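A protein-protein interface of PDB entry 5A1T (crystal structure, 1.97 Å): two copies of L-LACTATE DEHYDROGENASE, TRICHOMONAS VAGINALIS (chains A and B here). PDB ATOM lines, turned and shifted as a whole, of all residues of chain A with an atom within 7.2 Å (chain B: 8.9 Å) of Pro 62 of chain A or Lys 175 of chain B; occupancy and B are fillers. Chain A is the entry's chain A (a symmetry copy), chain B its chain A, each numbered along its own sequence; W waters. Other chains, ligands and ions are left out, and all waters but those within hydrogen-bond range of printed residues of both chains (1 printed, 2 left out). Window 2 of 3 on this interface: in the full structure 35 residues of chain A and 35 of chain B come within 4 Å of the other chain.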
ATOM      1  N   ALA A  25      31.236   2.184 -19.578  1.00  0.00           N
ATOM      2  CA  ALA A  25      29.795   2.121 -19.794  1.00  0.00           C
ATOM      3  C   ALA A  25      29.288   0.683 -19.779  1.00  0.00           C
ATOM      4  O   ALA A  25      28.129   0.434 -19.447  1.00  0.00           O
ATOM      5  CB  ALA A  25      29.432   2.790 -21.111  1.00  0.00           C
ATOM      6  N   SER A  26      30.154  -0.260 -20.140  1.00  0.00           N
ATOM      7  CA  SER A  26      29.787  -1.675 -20.136  1.00  0.00           C
ATOM      8  C   SER A  26      29.554  -2.175 -18.713  1.00  0.00           C
ATOM      9  O   SER A  26      28.949  -3.227 -18.510  1.00  0.00           O
ATOM     10  CB  SER A  26      30.869  -2.518 -20.817  1.00  0.00           C
ATOM     11  OG  SER A  26      32.051  -2.569 -20.037  1.00  0.00           O
ATOM     12  N   ASP A  32      27.350  -3.214 -10.751  1.00  0.00           N
ATOM     13  CA  ASP A  32      25.896  -3.072 -10.780  1.00  0.00           C
ATOM     14  C   ASP A  32      25.451  -1.612 -10.742  1.00  0.00           C
ATOM     15  O   ASP A  32      24.361  -1.278 -11.205  1.00  0.00           O
ATOM     16  CB  ASP A  32      25.264  -3.826  -9.606  1.00  0.00           C
ATOM     17  CG  ASP A  32      25.512  -5.321  -9.667  1.00  0.00           C
ATOM     18  OD1 ASP A  32      25.660  -5.860 -10.784  1.00  0.00           O
ATOM     19  OD2 ASP A  32      25.553  -5.958  -8.594  1.00  0.00           O
ATOM     20  N   GLN A  34      25.081   2.140 -11.793  1.00  0.00           N
ATOM     21  CA  GLN A  34      25.091   2.845 -13.067  1.00  0.00           C
ATOM     22  C   GLN A  34      26.179   3.908 -13.104  1.00  0.00           C
ATOM     23  O   GLN A  34      26.690   4.319 -12.062  1.00  0.00           O
ATOM     24  CB  GLN A  34      23.737   3.494 -13.335  1.00  0.00           C
ATOM     25  CG  GLN A  34      22.699   2.545 -13.886  1.00  0.00           C
ATOM     26  CD  GLN A  34      21.525   3.279 -14.490  1.00  0.00           C
ATOM     27  OE1 GLN A  34      20.975   4.197 -13.881  1.00  0.00           O
ATOM     28  NE2 GLN A  34      21.142   2.891 -15.699  1.00  0.00           N
ATOM     29  N   VAL A  35      26.522   4.348 -14.311  1.00  0.00           N
ATOM     30  CA  VAL A  35      27.535   5.378 -14.504  1.00  0.00           C
ATOM     31  C   VAL A  35      27.003   6.518 -15.370  1.00  0.00           C
ATOM     32  O   VAL A  35      26.258   6.290 -16.325  1.00  0.00           O
ATOM     33  CB  VAL A  35      28.811   4.799 -15.151  1.00  0.00           C
ATOM     34  CG1 VAL A  35      29.482   3.815 -14.207  1.00  0.00           C
ATOM     35  CG2 VAL A  35      28.491   4.130 -16.484  1.00  0.00           C
ATOM     36  N   CYS A  59      25.078   1.373 -28.283  1.00  0.00           N
ATOM     37  CA  CYS A  59      25.370   0.158 -27.530  1.00  0.00           C
ATOM     38  C   CYS A  59      24.188  -0.242 -26.655  1.00  0.00           C
ATOM     39  O   CYS A  59      24.055  -1.405 -26.269  1.00  0.00           O
ATOM     40  CB  CYS A  59      26.612   0.348 -26.662  1.00  0.00           C
ATOM     41  SG  CYS A  59      28.176   0.275 -27.557  1.00  0.00           S
ATOM     42  N   ALA A  60      23.336   0.730 -26.346  1.00  0.00           N
ATOM     43  CA  ALA A  60      22.195   0.511 -25.468  1.00  0.00           C
ATOM     44  C   ALA A  60      22.659  -0.062 -24.131  1.00  0.00           C
ATOM     45  O   ALA A  60      22.080  -1.023 -23.623  1.00  0.00           O
ATOM     46  CB  ALA A  60      21.184  -0.414 -26.130  1.00  0.00           C
ATOM     47  N   PHE A  61      23.716   0.530 -23.578  1.00  0.00           N
ATOM     48  CA  PHE A  61      24.264   0.099 -22.296  1.00  0.00           C
ATOM     49  C   PHE A  61      23.250   0.258 -21.168  1.00  0.00           C
ATOM     50  O   PHE A  61      22.819   1.374 -20.880  1.00  0.00           O
ATOM     51  CB  PHE A  61      25.522   0.899 -21.950  1.00  0.00           C
ATOM     52  CG  PHE A  61      26.728   0.533 -22.767  1.00  0.00           C
ATOM     53  CD1 PHE A  61      27.201  -0.769 -22.790  1.00  0.00           C
ATOM     54  CD2 PHE A  61      27.406   1.499 -23.490  1.00  0.00           C
ATOM     55  CE1 PHE A  61      28.317  -1.103 -23.533  1.00  0.00           C
ATOM     56  CE2 PHE A  61      28.524   1.173 -24.231  1.00  0.00           C
ATOM     57  CZ  PHE A  61      28.980  -0.129 -24.252  1.00  0.00           C
ATOM     58  N   PRO A  62      22.865  -0.853 -20.516  1.00  0.00           N
ATOM     59  CA  PRO A  62      21.946  -0.702 -19.383  1.00  0.00           C
ATOM     60  C   PRO A  62      22.610  -0.094 -18.146  1.00  0.00           C
ATOM     61  O   PRO A  62      21.908   0.380 -17.256  1.00  0.00           O
ATOM     62  CB  PRO A  62      21.493  -2.139 -19.107  1.00  0.00           C
ATOM     63  CG  PRO A  62      22.591  -2.988 -19.621  1.00  0.00           C
ATOM     64  CD  PRO A  62      23.126  -2.271 -20.823  1.00  0.00           C
ATOM     65  N   HIS A  63      23.941  -0.106 -18.096  1.00  0.00           N
ATOM     66  CA  HIS A  63      24.666   0.454 -16.958  1.00  0.00           C
ATOM     67  C   HIS A  63      24.958   1.941 -17.149  1.00  0.00           C
ATOM     68  O   HIS A  63      25.411   2.613 -16.223  1.00  0.00           O
ATOM     69  CB  HIS A  63      25.974  -0.307 -16.728  1.00  0.00           C
ATOM     70  CG  HIS A  63      25.780  -1.677 -16.154  1.00  0.00           C
ATOM     71  ND1 HIS A  63      25.944  -2.827 -16.897  1.00  0.00           N
ATOM     72  CD2 HIS A  63      25.434  -2.079 -14.909  1.00  0.00           C
ATOM     73  CE1 HIS A  63      25.710  -3.879 -16.132  1.00  0.00           C
ATOM     74  NE2 HIS A  63      25.398  -3.453 -14.922  1.00  0.00           N
ATOM     75  N   LEU A  64      24.699   2.450 -18.350  1.00  0.00           N
ATOM     76  CA  LEU A  64      24.885   3.870 -18.636  1.00  0.00           C
ATOM     77  C   LEU A  64      23.604   4.649 -18.354  1.00  0.00           C
ATOM     78  O   LEU A  64      22.641   4.582 -19.121  1.00  0.00           O
ATOM     79  CB  LEU A  64      25.319   4.070 -20.089  1.00  0.00           C
ATOM     80  CG  LEU A  64      25.686   5.500 -20.491  1.00  0.00           C
ATOM     81  CD1 LEU A  64      26.931   5.968 -19.753  1.00  0.00           C
ATOM     82  CD2 LEU A  64      25.886   5.601 -21.995  1.00  0.00           C
ATOM     83  N   ALA A  65      23.596   5.385 -17.246  1.00  0.00           N
ATOM     84  CA  ALA A  65      22.438   6.184 -16.859  1.00  0.00           C
ATOM     85  C   ALA A  65      22.260   7.360 -17.809  1.00  0.00           C
ATOM     86  O   ALA A  65      21.138   7.761 -18.121  1.00  0.00           O
ATOM     87  CB  ALA A  65      22.587   6.678 -15.430  1.00  0.00           C
ATOM     88  N   ASN B 160      20.187  -2.377 -31.360  1.00  0.00           N
ATOM     89  CA  ASN B 160      20.634  -1.548 -30.248  1.00  0.00           C
ATOM     90  C   ASN B 160      20.469  -0.070 -30.571  1.00  0.00           C
ATOM     91  O   ASN B 160      20.140   0.732 -29.698  1.00  0.00           O
ATOM     92  CB  ASN B 160      22.090  -1.863 -29.896  1.00  0.00           C
ATOM     93  CG  ASN B 160      22.238  -3.182 -29.153  1.00  0.00           C
ATOM     94  OD1 ASN B 160      21.304  -3.646 -28.496  1.00  0.00           O
ATOM     95  ND2 ASN B 160      23.415  -3.790 -29.251  1.00  0.00           N
ATOM     96  N   TYR B 163      16.729   0.455 -30.209  1.00  0.00           N
ATOM     97  CA  TYR B 163      16.330   0.432 -28.805  1.00  0.00           C
ATOM     98  C   TYR B 163      16.626   1.760 -28.115  1.00  0.00           C
ATOM     99  O   TYR B 163      15.774   2.297 -27.408  1.00  0.00           O
ATOM    100  CB  TYR B 163      17.027  -0.711 -28.062  1.00  0.00           C
ATOM    101  CG  TYR B 163      16.161  -1.942 -27.879  1.00  0.00           C
ATOM    102  CD1 TYR B 163      16.104  -2.928 -28.855  1.00  0.00           C
ATOM    103  CD2 TYR B 163      15.397  -2.113 -26.732  1.00  0.00           C
ATOM    104  CE1 TYR B 163      15.310  -4.052 -28.690  1.00  0.00           C
ATOM    105  CE2 TYR B 163      14.602  -3.232 -26.560  1.00  0.00           C
ATOM    106  CZ  TYR B 163      14.560  -4.198 -27.543  1.00  0.00           C
ATOM    107  OH  TYR B 163      13.769  -5.316 -27.379  1.00  0.00           O
ATOM    108  N   TYR B 164      17.825   2.298 -28.318  1.00  0.00           N
ATOM    109  CA  TYR B 164      18.188   3.546 -27.658  1.00  0.00           C
ATOM    110  C   TYR B 164      17.346   4.702 -28.181  1.00  0.00           C
ATOM    111  O   TYR B 164      16.889   5.543 -27.407  1.00  0.00           O
ATOM    112  CB  TYR B 164      19.673   3.869 -27.840  1.00  0.00           C
ATOM    113  CG  TYR B 164      20.104   5.046 -26.995  1.00  0.00           C
ATOM    114  CD1 TYR B 164      19.925   6.349 -27.441  1.00  0.00           C
ATOM    115  CD2 TYR B 164      20.657   4.854 -25.735  1.00  0.00           C
ATOM    116  CE1 TYR B 164      20.300   7.427 -26.667  1.00  0.00           C
ATOM    117  CE2 TYR B 164      21.037   5.929 -24.952  1.00  0.00           C
ATOM    118  CZ  TYR B 164      20.854   7.214 -25.422  1.00  0.00           C
ATOM    119  OH  TYR B 164      21.229   8.293 -24.655  1.00  0.00           O
ATOM    120  N   ALA B 167      13.821   4.480 -26.889  1.00  0.00           N
ATOM    121  CA  ALA B 167      13.862   4.715 -25.450  1.00  0.00           C
ATOM    122  C   ALA B 167      13.890   6.208 -25.127  1.00  0.00           C
ATOM    123  O   ALA B 167      13.221   6.662 -24.198  1.00  0.00           O
ATOM    124  CB  ALA B 167      15.073   4.019 -24.835  1.00  0.00           C
ATOM    125  N   VAL B 172      11.920   6.494 -21.233  1.00  0.00           N
ATOM    126  CA  VAL B 172      12.199   5.333 -20.394  1.00  0.00           C
ATOM    127  C   VAL B 172      13.566   4.752 -20.737  1.00  0.00           C
ATOM    128  O   VAL B 172      14.195   5.165 -21.710  1.00  0.00           O
ATOM    129  CB  VAL B 172      11.122   4.239 -20.558  1.00  0.00           C
ATOM    130  CG1 VAL B 172       9.767   4.749 -20.085  1.00  0.00           C
ATOM    131  CG2 VAL B 172      11.045   3.771 -22.006  1.00  0.00           C
ATOM    132  N   ASP B 173      14.025   3.796 -19.934  1.00  0.00           N
ATOM    133  CA  ASP B 173      15.301   3.135 -20.187  1.00  0.00           C
ATOM    134  C   ASP B 173      15.152   2.042 -21.240  1.00  0.00           C
ATOM    135  O   ASP B 173      14.048   1.563 -21.502  1.00  0.00           O
ATOM    136  CB  ASP B 173      15.868   2.536 -18.896  1.00  0.00           C
ATOM    137  CG  ASP B 173      16.329   3.595 -17.911  1.00  0.00           C
ATOM    138  OD1 ASP B 173      16.617   4.732 -18.338  1.00  0.00           O
ATOM    139  OD2 ASP B 173      16.411   3.283 -16.704  1.00  0.00           O
ATOM    140  N   VAL B 174      16.275   1.656 -21.838  1.00  0.00           N
ATOM    141  CA  VAL B 174      16.300   0.612 -22.856  1.00  0.00           C
ATOM    142  C   VAL B 174      15.692  -0.691 -22.346  1.00  0.00           C
ATOM    143  O   VAL B 174      14.939  -1.352 -23.060  1.00  0.00           O
ATOM    144  CB  VAL B 174      17.745   0.345 -23.335  1.00  0.00           C
ATOM    145  CG1 VAL B 174      17.855  -0.998 -24.067  1.00  0.00           C
ATOM    146  CG2 VAL B 174      18.215   1.479 -24.230  1.00  0.00           C
ATOM    147  N   LYS B 175      16.022  -1.051 -21.111  1.00  0.00           N
ATOM    148  CA  LYS B 175      15.552  -2.306 -20.532  1.00  0.00           C
ATOM    149  C   LYS B 175      14.030  -2.339 -20.412  1.00  0.00           C
ATOM    150  O   LYS B 175      13.436  -3.407 -20.281  1.00  0.00           O
ATOM    151  CB  LYS B 175      16.181  -2.530 -19.157  1.00  0.00           C
ATOM    152  CG  LYS B 175      17.695  -2.408 -19.135  1.00  0.00           C
ATOM    153  CD  LYS B 175      18.340  -3.544 -18.350  1.00  0.00           C
ATOM    154  CE  LYS B 175      18.360  -4.837 -19.154  1.00  0.00           C
ATOM    155  NZ  LYS B 175      19.132  -5.911 -18.468  1.00  0.00           N
ATOM    156  N   ASP B 176      13.404  -1.166 -20.462  1.00  0.00           N
ATOM    157  CA  ASP B 176      11.954  -1.057 -20.299  1.00  0.00           C
ATOM    158  C   ASP B 176      11.194  -1.211 -21.617  1.00  0.00           C
ATOM    159  O   ASP B 176       9.967  -1.156 -21.631  1.00  0.00           O
ATOM    160  CB  ASP B 176      11.597   0.284 -19.660  1.00  0.00           C
ATOM    161  CG  ASP B 176      12.109   0.408 -18.240  1.00  0.00           C
ATOM    162  OD1 ASP B 176      12.130  -0.609 -17.512  1.00  0.00           O
ATOM    163  OD2 ASP B 176      12.488   1.532 -17.847  1.00  0.00           O
ATOM    164  N   VAL B 177      11.921  -1.405 -22.714  1.00  0.00           N
ATOM    165  CA  VAL B 177      11.312  -1.585 -24.032  1.00  0.00           C
ATOM    166  C   VAL B 177      11.425  -3.051 -24.450  1.00  0.00           C
ATOM    167  O   VAL B 177      12.362  -3.740 -24.049  1.00  0.00           O
ATOM    168  CB  VAL B 177      11.980  -0.677 -25.088  1.00  0.00           C
ATOM    169  CG1 VAL B 177      11.321  -0.836 -26.447  1.00  0.00           C
ATOM    170  CG2 VAL B 177      11.918   0.782 -24.644  1.00  0.00           C
ATOM    171  N   HIS B 178      10.468  -3.520 -25.251  1.00  0.00           N
ATOM    172  CA  HIS B 178      10.422  -4.921 -25.666  1.00  0.00           C
ATOM    173  C   HIS B 178      10.028  -5.093 -27.128  1.00  0.00           C
ATOM    174  O   HIS B 178       9.283  -4.287 -27.682  1.00  0.00           O
ATOM    175  CB  HIS B 178       9.434  -5.700 -24.794  1.00  0.00           C
ATOM    176  CG  HIS B 178       9.646  -5.515 -23.325  1.00  0.00           C
ATOM    177  ND1 HIS B 178      10.462  -6.340 -22.585  1.00  0.00           N
ATOM    178  CD2 HIS B 178       9.148  -4.598 -22.463  1.00  0.00           C
ATOM    179  CE1 HIS B 178      10.457  -5.941 -21.325  1.00  0.00           C
ATOM    180  NE2 HIS B 178       9.669  -4.886 -21.224  1.00  0.00           N
ATOM    181  N   ASP B 179      10.536  -6.162 -27.735  1.00  0.00           N
ATOM    182  CA  ASP B 179      10.100  -6.618 -29.053  1.00  0.00           C
ATOM    183  C   ASP B 179      10.278  -5.593 -30.174  1.00  0.00           C
ATOM    184  O   ASP B 179       9.446  -5.506 -31.077  1.00  0.00           O
ATOM    185  CB  ASP B 179       8.633  -7.056 -28.986  1.00  0.00           C
ATOM    186  CG  ASP B 179       8.421  -8.242 -28.059  1.00  0.00           C
ATOM    187  OD1 ASP B 179       9.398  -8.977 -27.801  1.00  0.00           O
ATOM    188  OD2 ASP B 179       7.279  -8.446 -27.595  1.00  0.00           O
ATOM    189  N   THR B 198       6.602  -2.816 -27.550  1.00  0.00           N
ATOM    190  CA  THR B 198       5.906  -2.281 -26.389  1.00  0.00           C
ATOM    191  C   THR B 198       6.923  -1.737 -25.393  1.00  0.00           C
ATOM    192  O   THR B 198       8.128  -1.939 -25.551  1.00  0.00           O
ATOM    193  CB  THR B 198       5.042  -3.346 -25.683  1.00  0.00           C
ATOM    194  OG1 THR B 198       5.849  -4.488 -25.373  1.00  0.00           O
ATOM    195  CG2 THR B 198       3.872  -3.775 -26.554  1.00  0.00           C
ATOM    196  N   PHE B 199       6.430  -1.043 -24.373  1.00  0.00           N
ATOM    197  CA  PHE B 199       7.270  -0.591 -23.271  1.00  0.00           C
ATOM    198  C   PHE B 199       6.428  -0.499 -22.012  1.00  0.00           C
ATOM    199  O   PHE B 199       5.233  -0.203 -22.081  1.00  0.00           O
ATOM    200  CB  PHE B 199       7.914   0.761 -23.584  1.00  0.00           C
ATOM    201  CG  PHE B 199       6.965   1.922 -23.492  1.00  0.00           C
ATOM    202  CD1 PHE B 199       6.086   2.199 -24.524  1.00  0.00           C
ATOM    203  CD2 PHE B 199       6.955   2.738 -22.374  1.00  0.00           C
ATOM    204  CE1 PHE B 199       5.217   3.268 -24.443  1.00  0.00           C
ATOM    205  CE2 PHE B 199       6.086   3.809 -22.288  1.00  0.00           C
ATOM    206  CZ  PHE B 199       5.215   4.074 -23.324  1.00  0.00           C
ATOM    207  N   THR B 200       7.049  -0.762 -20.867  1.00  0.00           N
ATOM    208  CA  THR B 200       6.343  -0.722 -19.590  1.00  0.00           C
ATOM    209  C   THR B 200       6.912   0.377 -18.702  1.00  0.00           C
ATOM    210  O   THR B 200       8.125   0.581 -18.643  1.00  0.00           O
ATOM    211  CB  THR B 200       6.420  -2.069 -18.840  1.00  0.00           C
ATOM    212  OG1 THR B 200       7.550  -2.068 -17.960  1.00  0.00           O
ATOM    213  CG2 THR B 200       6.523  -3.236 -19.826  1.00  0.00           C
ATOM    214  N   LYS B 246      30.508  -4.540 -29.350  1.00  0.00           N
ATOM    215  CA  LYS B 246      29.608  -4.817 -28.239  1.00  0.00           C
ATOM    216  C   LYS B 246      28.452  -5.699 -28.699  1.00  0.00           C
ATOM    217  O   LYS B 246      28.087  -6.664 -28.026  1.00  0.00           O
ATOM    218  CB  LYS B 246      29.079  -3.507 -27.646  1.00  0.00           C
ATOM    219  CG  LYS B 246      28.267  -3.664 -26.372  1.00  0.00           C
ATOM    220  CD  LYS B 246      26.778  -3.830 -26.655  1.00  0.00           C
ATOM    221  CE  LYS B 246      25.980  -3.891 -25.365  1.00  0.00           C
ATOM    222  NZ  LYS B 246      24.522  -4.068 -25.616  1.00  0.00           N
ATOM    223  N   GLN B 250      27.685  -9.487 -27.583  1.00  0.00           N
ATOM    224  CA  GLN B 250      26.338  -9.717 -27.077  1.00  0.00           C
ATOM    225  C   GLN B 250      25.662 -10.825 -27.875  1.00  0.00           C
ATOM    226  O   GLN B 250      25.054 -11.733 -27.306  1.00  0.00           O
ATOM    227  CB  GLN B 250      25.513  -8.431 -27.148  1.00  0.00           C
ATOM    228  CG  GLN B 250      24.090  -8.579 -26.643  1.00  0.00           C
ATOM    229  CD  GLN B 250      23.329  -7.271 -26.671  1.00  0.00           C
ATOM    230  OE1 GLN B 250      23.804  -6.273 -27.215  1.00  0.00           O
ATOM    231  NE2 GLN B 250      22.142  -7.265 -26.078  1.00  0.00           N
ATOM    232  N   ALA B 260      17.597 -14.467 -22.378  1.00  0.00           N
ATOM    233  CA  ALA B 260      16.849 -14.284 -21.139  1.00  0.00           C
ATOM    234  C   ALA B 260      15.345 -14.309 -21.408  1.00  0.00           C
ATOM    235  O   ALA B 260      14.919 -14.227 -22.559  1.00  0.00           O
ATOM    236  CB  ALA B 260      17.253 -12.975 -20.480  1.00  0.00           C
ATOM    237  N   PRO B 261      14.531 -14.433 -20.345  1.00  0.00           N
ATOM    238  CA  PRO B 261      13.075 -14.463 -20.530  1.00  0.00           C
ATOM    239  C   PRO B 261      12.543 -13.220 -21.238  1.00  0.00           C
ATOM    240  O   PRO B 261      12.802 -12.101 -20.798  1.00  0.00           O
ATOM    241  CB  PRO B 261      12.541 -14.544 -19.096  1.00  0.00           C
ATOM    242  CG  PRO B 261      13.645 -15.165 -18.316  1.00  0.00           C
ATOM    243  CD  PRO B 261      14.907 -14.644 -18.934  1.00  0.00           C
ATOM    244  N   GLY B 262      11.812 -13.427 -22.328  1.00  0.00           N
ATOM    245  CA  GLY B 262      11.224 -12.332 -23.079  1.00  0.00           C
ATOM    246  C   GLY B 262      12.200 -11.617 -23.993  1.00  0.00           C
ATOM    247  O   GLY B 262      11.811 -10.708 -24.730  1.00  0.00           O
ATOM    248  N   GLU B 263      13.466 -12.019 -23.953  1.00  0.00           N
ATOM    249  CA  GLU B 263      14.492 -11.374 -24.765  1.00  0.00           C
ATOM    250  C   GLU B 263      14.374 -11.792 -26.226  1.00  0.00           C
ATOM    251  O   GLU B 263      14.313 -12.984 -26.538  1.00  0.00           O
ATOM    252  CB  GLU B 263      15.891 -11.705 -24.235  1.00  0.00           C
ATOM    253  CG  GLU B 263      17.019 -11.037 -25.015  1.00  0.00           C
ATOM    254  CD  GLU B 263      18.377 -11.215 -24.359  1.00  0.00           C
ATOM    255  OE1 GLU B 263      18.634 -12.292 -23.780  1.00  0.00           O
ATOM    256  OE2 GLU B 263      19.192 -10.271 -24.421  1.00  0.00           O
HETATM  257  O   HOH W   1      18.821   6.844 -17.211  1.00  0.00           O
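The side-chain amino group of Lys 246 of chain B lies within hydrogen-bond range of the backbone carbonyl oxygen of Cys 59 of chain A (2.8 Å).
The side-chain amide oxygen (OE1) of Gln 250 of chain B is in hydrogen-bond range of the side-chain amide nitrogen (ND2) of Asn 160 of chain B, at 3.2 Å. NZ of Lys 246 of chain B is in hydrogen-bond range of OE1 of Gln 250 of chain B (2.8 Å). The side-chain amide nitrogen (NE2) of Gln 34 of chain A lies within hydrogen-bond range of the backbone carbonyl oxygen (O) of Pro 62 of chain A, at 3.1 Å.
Among the printed residues, merely in contact across the chains: Pro 62 of chain A with Lys 175 of chain B, Phe 61 of chain A with Lys 246 of chain B, Cys 59 of chain A with Asn 160 of chain B, Ala 60 of chain A with Asn 160 of chain B and Ala 60 of chain A with Val 174 of chain B.
Of the printed residues of chain B, Ala 60 of chain A touches Asn 160 (3.9 Å) and Val 174 (3.96 Å). Of the printed residues of chain B, Phe 61 of chain A touches Lys 246 (3.8 Å). Pro 62 of chain A touches just one residue of chain B: Lys 175 (3.5 Å). Printed residues of chain A within 4 Å of Asn 160 of chain B: Cys 59 and Ala 60. Printed residues of chain A within 4 Å of Val 174 of chain B: Ala 60 (3.96 Å). Of chain A, only Pro 62 comes within 4 Å of Lys 175 of chain B. Printed residues of chain A within 4 Å of Lys 246 of chain B: Cys 59 (2.8 Å) and Phe 61 (3.8 Å). The nearest residue of chain B that does not touch Pro 62 of chain A is Lys 246 of chain B (5.3 Å). The nearest residue of chain A that does not touch Lys 175 of chain B is Ala 60 of chain A (6.4 Å).
Of the 12 printed residues of chain A, 4 touch a printed residue of chain B. Of the 21 printed residues of chain B, 4 touch a printed residue of chain A. Printed residues of chain B that touch a printed residue of chain A: Asn 160, Val 174, Lys 175 and Lys 246. Hydrophobic or aromatic side chains of chain B that line the printed part of chain A: Val 174. Along chain B the printed residues that touch a printed residue of chain A span positions 160 to 246. Among the printed residues, 6 pairs touch across the chains. Among the printed residues, no Asp or Glu carboxylate lies within 4 Å of a Lys or Arg side-chain nitrogen of the other chain.
No position is printed for both chains.
Water W1 lies within hydrogen-bond range of the backbone carbonyl oxygen (O) of Ala 65 of chain A and the side-chain carboxylate (OD1) of Asp 173 of chain B.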
